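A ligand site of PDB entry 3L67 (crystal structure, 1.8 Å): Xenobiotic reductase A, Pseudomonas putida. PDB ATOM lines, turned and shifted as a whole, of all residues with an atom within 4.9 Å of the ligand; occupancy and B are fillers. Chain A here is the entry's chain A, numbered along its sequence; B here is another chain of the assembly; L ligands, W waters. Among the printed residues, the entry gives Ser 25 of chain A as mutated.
A ring nitrogen (ND1) of His 181 sits close to an oxygen (O1) of the ligand, at 3.5 Å.
An oxygen (O2) of the ligand is in hydrogen-bond range of the side-chain hydroxyl (OG) of Ser 25 (2.8 Å).
The guanidinium group (NH1) of Arg 231 is in hydrogen-bond range of an oxygen (O4) of the ligand (2.9 Å).
O6 of the ligand is in hydrogen-bond range of N of Trp 302 (3.4 Å).
A nitrogen (N3) of the ligand lies within hydrogen-bond range of the backbone NH (N) of Ser 25 (2.8 Å).
The backbone NH of Ala 57 is in hydrogen-bond range of an oxygen (O2) of the ligand (3.2 Å).
The backbone carbonyl oxygen of Pro 23 is in hydrogen-bond range of an oxygen (O3) of the ligand (2.9 Å).
NE of Arg 326 is in salt-bridge range of O7 of the ligand.
A ring nitrogen (NE2) of His 178 is in hydrogen-bond range of an oxygen (O1) of the ligand.
An oxygen (O8) of the ligand lies within hydrogen-bond range of the backbone NH (N) of Gly 303, at 2.9 Å.
The backbone NH of Gly 325 is in hydrogen-bond range of an oxygen (O9) of the ligand (2.7 Å).
The backbone NH (N) of Arg 326 sits at hydrogen-bond distance from an oxygen (O7) of the ligand, 2.9 Å away.
The side-chain amide oxygen (OE1) of Gln 99 lies within hydrogen-bond range of a nitrogen (N2) of the ligand (2.9 Å).
The side-chain amide nitrogen of Gln 99 sits at hydrogen-bond distance from the side-chain carboxylate of Glu 176, 2.7 Å away.
OE1 of Gln 99 sits close to N of Ala 57 (3.4 Å).
The backbone carbonyl oxygen (O) of Met 24 sits close to the side-chain amide oxygen (OE1) of Gln 26.
The backbone carbonyl oxygen (O) of Pro 354 of chain B lies close to the indole nitrogen (NE1) of Trp 358 of chain B, 3.5 Å away.
Pro 22 touches the ligand.
CA of Met 24 touches N3 of the ligand, 3.3 Å away.
Ala 301 touches the ligand (CB to O6, 3.5 Å).
Val 324 touches the ligand.
Leu 329 touches the ligand (CD1 to C7, 3.9 Å).
NE1 of Trp 358 of chain B touches C7 of the ligand, at 3.2 Å.
17 residues have an atom within 4 Å of the ligand: Pro 22, Pro 23, Met 24, Ser 25, Ala 57, Gln 99, His 178, His 181, Arg 231, Ala 301, Trp 302, Gly 303, Val 324, Gly 325, Arg 326, Leu 329 and Trp 358 of chain B.
Water W2 bridges O9 of the ligand (2.8 Å) and N of Arg 326 (3.4 Å).
Water W1 lies within hydrogen-bond range of O8 of the ligand (3.0 Å) and NH2 of Arg 326 (3.3 Å).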
ATOM      1  N   PRO A  22      -7.213 -17.786   8.373  1.00  0.00           N
ATOM      2  CA  PRO A  22      -6.311 -18.654   7.618  1.00  0.00           C
ATOM      3  C   PRO A  22      -6.827 -18.817   6.193  1.00  0.00           C
ATOM      4  O   PRO A  22      -7.997 -18.521   5.921  1.00  0.00           O
ATOM      5  CB  PRO A  22      -6.385 -19.986   8.370  1.00  0.00           C
ATOM      6  CG  PRO A  22      -7.749 -19.959   9.015  1.00  0.00           C
ATOM      7  CD  PRO A  22      -7.954 -18.525   9.408  1.00  0.00           C
ATOM      8  N   PRO A  23      -5.963 -19.276   5.280  1.00  0.00           N
ATOM      9  CA  PRO A  23      -6.441 -19.499   3.917  1.00  0.00           C
ATOM     10  C   PRO A  23      -7.535 -20.561   3.887  1.00  0.00           C
ATOM     11  O   PRO A  23      -7.363 -21.644   4.458  1.00  0.00           O
ATOM     12  CB  PRO A  23      -5.190 -19.989   3.182  1.00  0.00           C
ATOM     13  CG  PRO A  23      -4.274 -20.514   4.265  1.00  0.00           C
ATOM     14  CD  PRO A  23      -4.536 -19.632   5.444  1.00  0.00           C
ATOM     15  N   MET A  24      -8.643 -20.251   3.224  1.00  0.00           N
ATOM     16  CA  MET A  24      -9.752 -21.182   3.091  1.00  0.00           C
ATOM     17  C   MET A  24     -10.287 -21.266   1.651  1.00  0.00           C
ATOM     18  O   MET A  24     -11.095 -20.437   1.212  1.00  0.00           O
ATOM     19  CB  MET A  24     -10.868 -20.809   4.086  1.00  0.00           C
ATOM     20  CG  MET A  24     -10.598 -21.256   5.505  1.00  0.00           C
ATOM     21  SD  MET A  24     -11.891 -20.841   6.677  1.00  0.00           S
ATOM     22  CE  MET A  24     -11.778 -19.049   6.696  1.00  0.00           C
ATOM     23  N   SER A  25      -9.812 -22.273   0.925  1.00  0.00           N
ATOM     24  CA  SER A  25     -10.295 -22.554  -0.430  1.00  0.00           C
ATOM     25  C   SER A  25     -11.815 -22.478  -0.534  1.00  0.00           C
ATOM     26  O   SER A  25     -12.531 -23.011   0.316  1.00  0.00           O
ATOM     27  CB  SER A  25      -9.817 -23.934  -0.891  1.00  0.00           C
ATOM     28  OG  SER A  25      -8.421 -23.948  -1.079  1.00  0.00           O
ATOM     29  N   GLN A  26     -12.296 -21.834  -1.586  1.00  0.00           N
ATOM     30  CA  GLN A  26     -13.725 -21.623  -1.800  1.00  0.00           C
ATOM     31  C   GLN A  26     -14.272 -22.448  -2.978  1.00  0.00           C
ATOM     32  O   GLN A  26     -15.475 -22.640  -3.110  1.00  0.00           O
ATOM     33  CB  GLN A  26     -14.014 -20.128  -2.046  1.00  0.00           C
ATOM     34  CG  GLN A  26     -13.627 -19.237  -0.866  1.00  0.00           C
ATOM     35  CD  GLN A  26     -14.410 -19.565   0.389  1.00  0.00           C
ATOM     36  OE1 GLN A  26     -13.880 -20.155   1.330  1.00  0.00           O
ATOM     37  NE2 GLN A  26     -15.685 -19.181   0.407  1.00  0.00           N
ATOM     38  N   TYR A  27     -13.382 -22.935  -3.820  1.00  0.00           N
ATOM     39  CA  TYR A  27     -13.763 -23.776  -4.944  1.00  0.00           C
ATOM     40  C   TYR A  27     -14.772 -23.096  -5.860  1.00  0.00           C
ATOM     41  O   TYR A  27     -15.577 -23.780  -6.484  1.00  0.00           O
ATOM     42  CB  TYR A  27     -14.308 -25.121  -4.453  1.00  0.00           C
ATOM     43  CG  TYR A  27     -13.405 -25.765  -3.446  1.00  0.00           C
ATOM     44  CD1 TYR A  27     -12.341 -26.566  -3.846  1.00  0.00           C
ATOM     45  CD2 TYR A  27     -13.584 -25.540  -2.082  1.00  0.00           C
ATOM     46  CE1 TYR A  27     -11.491 -27.142  -2.934  1.00  0.00           C
ATOM     47  CE2 TYR A  27     -12.727 -26.118  -1.147  1.00  0.00           C
ATOM     48  CZ  TYR A  27     -11.703 -26.927  -1.582  1.00  0.00           C
ATOM     49  OH  TYR A  27     -10.853 -27.509  -0.683  1.00  0.00           O
ATOM     50  N   GLU A  56      -7.113 -17.686   0.171  1.00  0.00           N
ATOM     51  CA  GLU A  56      -7.016 -19.127  -0.039  1.00  0.00           C
ATOM     52  C   GLU A  56      -5.837 -19.601  -0.918  1.00  0.00           C
ATOM     53  O   GLU A  56      -5.294 -18.834  -1.710  1.00  0.00           O
ATOM     54  CB  GLU A  56      -8.307 -19.615  -0.695  1.00  0.00           C
ATOM     55  CG  GLU A  56      -8.496 -19.097  -2.109  1.00  0.00           C
ATOM     56  CD  GLU A  56      -9.919 -19.215  -2.583  1.00  0.00           C
ATOM     57  OE1 GLU A  56     -10.296 -20.260  -3.159  1.00  0.00           O
ATOM     58  OE2 GLU A  56     -10.683 -18.264  -2.349  1.00  0.00           O
ATOM     59  N   ALA A  57      -5.462 -20.868  -0.789  1.00  0.00           N
ATOM     60  CA  ALA A  57      -4.457 -21.480  -1.656  1.00  0.00           C
ATOM     61  C   ALA A  57      -4.686 -21.049  -3.105  1.00  0.00           C
ATOM     62  O   ALA A  57      -5.730 -21.319  -3.688  1.00  0.00           O
ATOM     63  CB  ALA A  57      -4.508 -22.988  -1.562  1.00  0.00           C
ATOM     64  N   GLN A  99      -1.909 -17.042   0.114  1.00  0.00           N
ATOM     65  CA  GLN A  99      -1.144 -18.282   0.180  1.00  0.00           C
ATOM     66  C   GLN A  99      -0.998 -18.810  -1.243  1.00  0.00           C
ATOM     67  O   GLN A  99      -2.001 -19.016  -1.933  1.00  0.00           O
ATOM     68  CB  GLN A  99      -1.853 -19.312   1.077  1.00  0.00           C
ATOM     69  CG  GLN A  99      -1.142 -20.649   1.111  1.00  0.00           C
ATOM     70  CD  GLN A  99      -1.990 -21.747   1.713  1.00  0.00           C
ATOM     71  OE1 GLN A  99      -3.029 -22.096   1.176  1.00  0.00           O
ATOM     72  NE2 GLN A  99      -1.545 -22.290   2.855  1.00  0.00           N
ATOM     73  N   GLU A 176       2.343 -16.339   1.925  1.00  0.00           N
ATOM     74  CA  GLU A 176       2.470 -17.616   2.614  1.00  0.00           C
ATOM     75  C   GLU A 176       2.677 -18.733   1.623  1.00  0.00           C
ATOM     76  O   GLU A 176       1.821 -19.006   0.772  1.00  0.00           O
ATOM     77  CB  GLU A 176       1.235 -17.906   3.467  1.00  0.00           C
ATOM     78  CG  GLU A 176       1.352 -19.190   4.295  1.00  0.00           C
ATOM     79  CD  GLU A 176       0.092 -19.536   5.063  1.00  0.00           C
ATOM     80  OE1 GLU A 176      -0.179 -18.873   6.091  1.00  0.00           O
ATOM     81  OE2 GLU A 176      -0.619 -20.466   4.657  1.00  0.00           O
ATOM     82  N   HIS A 178       2.798 -22.501   0.632  1.00  0.00           N
ATOM     83  CA  HIS A 178       2.036 -23.649   1.111  1.00  0.00           C
ATOM     84  C   HIS A 178       2.863 -24.919   1.023  1.00  0.00           C
ATOM     85  O   HIS A 178       2.780 -25.669   0.052  1.00  0.00           O
ATOM     86  CB  HIS A 178       0.749 -23.804   0.298  1.00  0.00           C
ATOM     87  CG  HIS A 178      -0.273 -24.662   0.971  1.00  0.00           C
ATOM     88  ND1 HIS A 178       0.023 -25.421   2.086  1.00  0.00           N
ATOM     89  CD2 HIS A 178      -1.581 -24.880   0.704  1.00  0.00           C
ATOM     90  CE1 HIS A 178      -1.062 -26.071   2.466  1.00  0.00           C
ATOM     91  NE2 HIS A 178      -2.046 -25.757   1.645  1.00  0.00           N
ATOM     92  N   HIS A 181       0.082 -29.917   4.373  1.00  0.00           N
ATOM     93  CA  HIS A 181      -1.130 -30.642   3.992  1.00  0.00           C
ATOM     94  C   HIS A 181      -0.976 -31.610   2.829  1.00  0.00           C
ATOM     95  O   HIS A 181      -1.932 -31.863   2.074  1.00  0.00           O
ATOM     96  CB  HIS A 181      -2.297 -29.669   3.740  1.00  0.00           C
ATOM     97  CG  HIS A 181      -2.578 -28.750   4.897  1.00  0.00           C
ATOM     98  ND1 HIS A 181      -3.346 -27.622   4.783  1.00  0.00           N
ATOM     99  CD2 HIS A 181      -2.163 -28.794   6.187  1.00  0.00           C
ATOM    100  CE1 HIS A 181      -3.408 -27.012   5.949  1.00  0.00           C
ATOM    101  NE2 HIS A 181      -2.696 -27.696   6.816  1.00  0.00           N
ATOM    102  N   ARG A 231       3.511 -22.231   5.382  1.00  0.00           N
ATOM    103  CA  ARG A 231       2.753 -23.186   6.166  1.00  0.00           C
ATOM    104  C   ARG A 231       3.425 -24.527   5.990  1.00  0.00           C
ATOM    105  O   ARG A 231       3.818 -24.887   4.885  1.00  0.00           O
ATOM    106  CB  ARG A 231       1.283 -23.235   5.710  1.00  0.00           C
ATOM    107  CG  ARG A 231       0.370 -23.820   6.781  1.00  0.00           C
ATOM    108  CD  ARG A 231      -1.123 -23.608   6.497  1.00  0.00           C
ATOM    109  NE  ARG A 231      -1.851 -23.648   7.764  1.00  0.00           N
ATOM    110  CZ  ARG A 231      -3.163 -23.529   7.927  1.00  0.00           C
ATOM    111  NH1 ARG A 231      -3.681 -23.582   9.150  1.00  0.00           N
ATOM    112  NH2 ARG A 231      -3.963 -23.373   6.883  1.00  0.00           N
ATOM    113  N   ALA A 301      -3.872 -23.317  13.863  1.00  0.00           N
ATOM    114  CA  ALA A 301      -5.321 -23.333  13.826  1.00  0.00           C
ATOM    115  C   ALA A 301      -5.911 -24.642  14.332  1.00  0.00           C
ATOM    116  O   ALA A 301      -5.182 -25.572  14.688  1.00  0.00           O
ATOM    117  CB  ALA A 301      -5.799 -23.042  12.402  1.00  0.00           C
ATOM    118  N   TRP A 302      -7.246 -24.658  14.389  1.00  0.00           N
ATOM    119  CA  TRP A 302      -8.108 -25.797  14.681  1.00  0.00           C
ATOM    120  C   TRP A 302      -8.794 -25.707  16.057  1.00  0.00           C
ATOM    121  O   TRP A 302      -8.243 -26.150  17.056  1.00  0.00           O
ATOM    122  CB  TRP A 302      -7.464 -27.178  14.481  1.00  0.00           C
ATOM    123  CG  TRP A 302      -8.497 -28.270  14.653  1.00  0.00           C
ATOM    124  CD1 TRP A 302      -8.906 -28.831  15.830  1.00  0.00           C
ATOM    125  CD2 TRP A 302      -9.289 -28.890  13.625  1.00  0.00           C
ATOM    126  NE1 TRP A 302      -9.882 -29.778  15.599  1.00  0.00           N
ATOM    127  CE2 TRP A 302     -10.138 -29.829  14.250  1.00  0.00           C
ATOM    128  CE3 TRP A 302      -9.348 -28.736  12.232  1.00  0.00           C
ATOM    129  CZ2 TRP A 302     -11.033 -30.616  13.528  1.00  0.00           C
ATOM    130  CZ3 TRP A 302     -10.247 -29.531  11.528  1.00  0.00           C
ATOM    131  CH2 TRP A 302     -11.074 -30.452  12.176  1.00  0.00           C
ATOM    132  N   GLY A 303      -9.984 -25.124  16.068  1.00  0.00           N
ATOM    133  CA  GLY A 303     -10.796 -25.038  17.270  1.00  0.00           C
ATOM    134  C   GLY A 303     -10.530 -23.817  18.117  1.00  0.00           C
ATOM    135  O   GLY A 303     -10.865 -23.795  19.291  1.00  0.00           O
ATOM    136  N   PHE A 304      -9.914 -22.795  17.539  1.00  0.00           N
ATOM    137  CA  PHE A 304      -9.663 -21.558  18.289  1.00  0.00           C
ATOM    138  C   PHE A 304     -10.810 -20.574  18.147  1.00  0.00           C
ATOM    139  O   PHE A 304     -10.757 -19.453  18.634  1.00  0.00           O
ATOM    140  CB  PHE A 304      -8.342 -20.904  17.866  1.00  0.00           C
ATOM    141  CG  PHE A 304      -7.116 -21.636  18.345  1.00  0.00           C
ATOM    142  CD1 PHE A 304      -6.677 -21.502  19.650  1.00  0.00           C
ATOM    143  CD2 PHE A 304      -6.405 -22.447  17.480  1.00  0.00           C
ATOM    144  CE1 PHE A 304      -5.542 -22.164  20.092  1.00  0.00           C
ATOM    145  CE2 PHE A 304      -5.280 -23.111  17.908  1.00  0.00           C
ATOM    146  CZ  PHE A 304      -4.840 -22.972  19.226  1.00  0.00           C
ATOM    147  N   SER A 323      -5.069 -18.296  14.375  1.00  0.00           N
ATOM    148  CA  SER A 323      -5.804 -18.460  13.121  1.00  0.00           C
ATOM    149  C   SER A 323      -7.178 -19.077  13.369  1.00  0.00           C
ATOM    150  O   SER A 323      -7.287 -20.118  14.024  1.00  0.00           O
ATOM    151  CB  SER A 323      -5.008 -19.315  12.146  1.00  0.00           C
ATOM    152  OG  SER A 323      -3.834 -18.630  11.723  1.00  0.00           O
ATOM    153  N   VAL A 324      -8.226 -18.445  12.834  1.00  0.00           N
ATOM    154  CA  VAL A 324      -9.624 -18.837  13.094  1.00  0.00           C
ATOM    155  C   VAL A 324     -10.362 -19.002  11.772  1.00  0.00           C
ATOM    156  O   VAL A 324     -10.588 -18.038  11.049  1.00  0.00           O
ATOM    157  CB  VAL A 324     -10.333 -17.787  13.950  1.00  0.00           C
ATOM    158  CG1 VAL A 324     -11.767 -18.204  14.280  1.00  0.00           C
ATOM    159  CG2 VAL A 324      -9.533 -17.556  15.248  1.00  0.00           C
ATOM    160  N   GLY A 325     -10.706 -20.244  11.432  1.00  0.00           N
ATOM    161  CA  GLY A 325     -11.197 -20.546  10.099  1.00  0.00           C
ATOM    162  C   GLY A 325     -12.707 -20.663   9.994  1.00  0.00           C
ATOM    163  O   GLY A 325     -13.396 -19.726   9.584  1.00  0.00           O
ATOM    164  N   ARG A 326     -13.213 -21.831  10.380  1.00  0.00           N
ATOM    165  CA  ARG A 326     -14.613 -22.170  10.173  1.00  0.00           C
ATOM    166  C   ARG A 326     -15.567 -21.210  10.877  1.00  0.00           C
ATOM    167  O   ARG A 326     -16.656 -20.947  10.376  1.00  0.00           O
ATOM    168  CB  ARG A 326     -14.877 -23.622  10.596  1.00  0.00           C
ATOM    169  CG  ARG A 326     -14.519 -24.648   9.512  1.00  0.00           C
ATOM    170  CD  ARG A 326     -14.546 -26.058  10.052  1.00  0.00           C
ATOM    171  NE  ARG A 326     -13.503 -26.253  11.071  1.00  0.00           N
ATOM    172  CZ  ARG A 326     -13.140 -27.442  11.542  1.00  0.00           C
ATOM    173  NH1 ARG A 326     -13.735 -28.540  11.104  1.00  0.00           N
ATOM    174  NH2 ARG A 326     -12.177 -27.516  12.460  1.00  0.00           N
ATOM    175  N   LEU A 329     -16.527 -18.558   8.507  1.00  0.00           N
ATOM    176  CA  LEU A 329     -17.511 -18.981   7.530  1.00  0.00           C
ATOM    177  C   LEU A 329     -18.910 -18.936   8.152  1.00  0.00           C
ATOM    178  O   LEU A 329     -19.877 -18.608   7.486  1.00  0.00           O
ATOM    179  CB  LEU A 329     -17.209 -20.384   7.006  1.00  0.00           C
ATOM    180  CG  LEU A 329     -15.855 -20.686   6.352  1.00  0.00           C
ATOM    181  CD1 LEU A 329     -15.765 -22.158   5.972  1.00  0.00           C
ATOM    182  CD2 LEU A 329     -15.662 -19.817   5.144  1.00  0.00           C
ATOM    183  N   PRO B 354     -19.938 -23.287  -0.424  1.00  0.00           N
ATOM    184  CA  PRO B 354     -18.559 -23.096   0.060  1.00  0.00           C
ATOM    185  C   PRO B 354     -18.506 -22.838   1.560  1.00  0.00           C
ATOM    186  O   PRO B 354     -17.428 -22.911   2.139  1.00  0.00           O
ATOM    187  CB  PRO B 354     -18.071 -21.864  -0.715  1.00  0.00           C
ATOM    188  CG  PRO B 354     -18.953 -21.815  -1.924  1.00  0.00           C
ATOM    189  CD  PRO B 354     -20.289 -22.307  -1.458  1.00  0.00           C
ATOM    190  N   TRP B 358     -18.771 -27.196   5.174  1.00  0.00           N
ATOM    191  CA  TRP B 358     -17.815 -27.337   6.262  1.00  0.00           C
ATOM    192  C   TRP B 358     -18.453 -27.150   7.625  1.00  0.00           C
ATOM    193  O   TRP B 358     -17.851 -27.476   8.640  1.00  0.00           O
ATOM    194  CB  TRP B 358     -16.669 -26.332   6.080  1.00  0.00           C
ATOM    195  CG  TRP B 358     -16.113 -26.368   4.695  1.00  0.00           C
ATOM    196  CD1 TRP B 358     -16.484 -25.587   3.638  1.00  0.00           C
ATOM    197  CD2 TRP B 358     -15.117 -27.269   4.204  1.00  0.00           C
ATOM    198  NE1 TRP B 358     -15.773 -25.931   2.526  1.00  0.00           N
ATOM    199  CE2 TRP B 358     -14.921 -26.966   2.834  1.00  0.00           C
ATOM    200  CE3 TRP B 358     -14.368 -28.296   4.779  1.00  0.00           C
ATOM    201  CZ2 TRP B 358     -14.006 -27.644   2.051  1.00  0.00           C
ATOM    202  CZ3 TRP B 358     -13.451 -28.970   3.987  1.00  0.00           C
ATOM    203  CH2 TRP B 358     -13.280 -28.636   2.635  1.00  0.00           C
HETATM  204  N1  LIG L   1      -5.642 -24.633   4.630  1.00  0.00           N
HETATM  205  C1  LIG L   1      -4.671 -24.161   3.770  1.00  0.00           C
HETATM  206  O1  LIG L   1      -3.486 -24.218   4.103  1.00  0.00           O
HETATM  207  N2  LIG L   1      -5.017 -23.688   2.522  1.00  0.00           N
HETATM  208  C2  LIG L   1      -6.331 -23.770   2.089  1.00  0.00           C
HETATM  209  O2  LIG L   1      -6.666 -23.249   1.019  1.00  0.00           O
HETATM  210  C3  LIG L   1      -7.307 -24.255   2.954  1.00  0.00           C
HETATM  211  N3  LIG L   1      -8.631 -24.282   2.552  1.00  0.00           N
HETATM  212  C4  LIG L   1      -9.628 -24.510   3.477  1.00  0.00           C
HETATM  213  C5  LIG L   1     -10.952 -24.453   3.089  1.00  0.00           C
HETATM  214  C6  LIG L   1     -11.959 -24.547   4.045  1.00  0.00           C
HETATM  215  C7  LIG L   1     -13.351 -24.137   3.702  1.00  0.00           C
HETATM  216  C8  LIG L   1     -11.631 -24.907   5.348  1.00  0.00           C
HETATM  217  C9  LIG L   1     -12.725 -25.096   6.377  1.00  0.00           C
HETATM  218  C10 LIG L   1     -10.299 -25.059   5.720  1.00  0.00           C
HETATM  219  C11 LIG L   1      -9.294 -24.890   4.773  1.00  0.00           C
HETATM  220  N4  LIG L   1      -7.964 -24.925   5.160  1.00  0.00           N
HETATM  221  C12 LIG L   1      -6.974 -24.560   4.259  1.00  0.00           C
HETATM  222  C13 LIG L   1      -7.604 -25.178   6.605  1.00  0.00           C
HETATM  223  C14 LIG L   1      -7.839 -23.900   7.413  1.00  0.00           C
HETATM  224  O3  LIG L   1      -6.907 -22.903   7.010  1.00  0.00           O
HETATM  225  C15 LIG L   1      -7.707 -24.159   8.924  1.00  0.00           C
HETATM  226  O4  LIG L   1      -6.415 -24.655   9.207  1.00  0.00           O
HETATM  227  C16 LIG L   1      -8.756 -25.168   9.405  1.00  0.00           C
HETATM  228  O5  LIG L   1     -10.038 -24.714   9.039  1.00  0.00           O
HETATM  229  C17 LIG L   1      -8.691 -25.362  10.927  1.00  0.00           C
HETATM  230  O6  LIG L   1      -9.053 -24.156  11.586  1.00  0.00           O
HETATM  231  P1  LIG L   1     -10.548 -23.942  12.180  1.00  0.00           P
HETATM  232  O7  LIG L   1     -11.546 -24.092  11.059  1.00  0.00           O
HETATM  233  O8  LIG L   1     -10.820 -24.975  13.245  1.00  0.00           O
HETATM  234  O9  LIG L   1     -10.658 -22.561  12.784  1.00  0.00           O
HETATM  235  O   HOH W   1     -13.481 -25.362  14.555  1.00  0.00           O
HETATM  236  O   HOH W   2     -13.076 -21.663  13.817  1.00  0.00           O
HETATM  237  O   HOH W   3      -8.743 -22.398  14.705  1.00  0.00           O
HETATM  238  O   HOH W   4     -10.820 -27.579   8.208  1.00  0.00           O
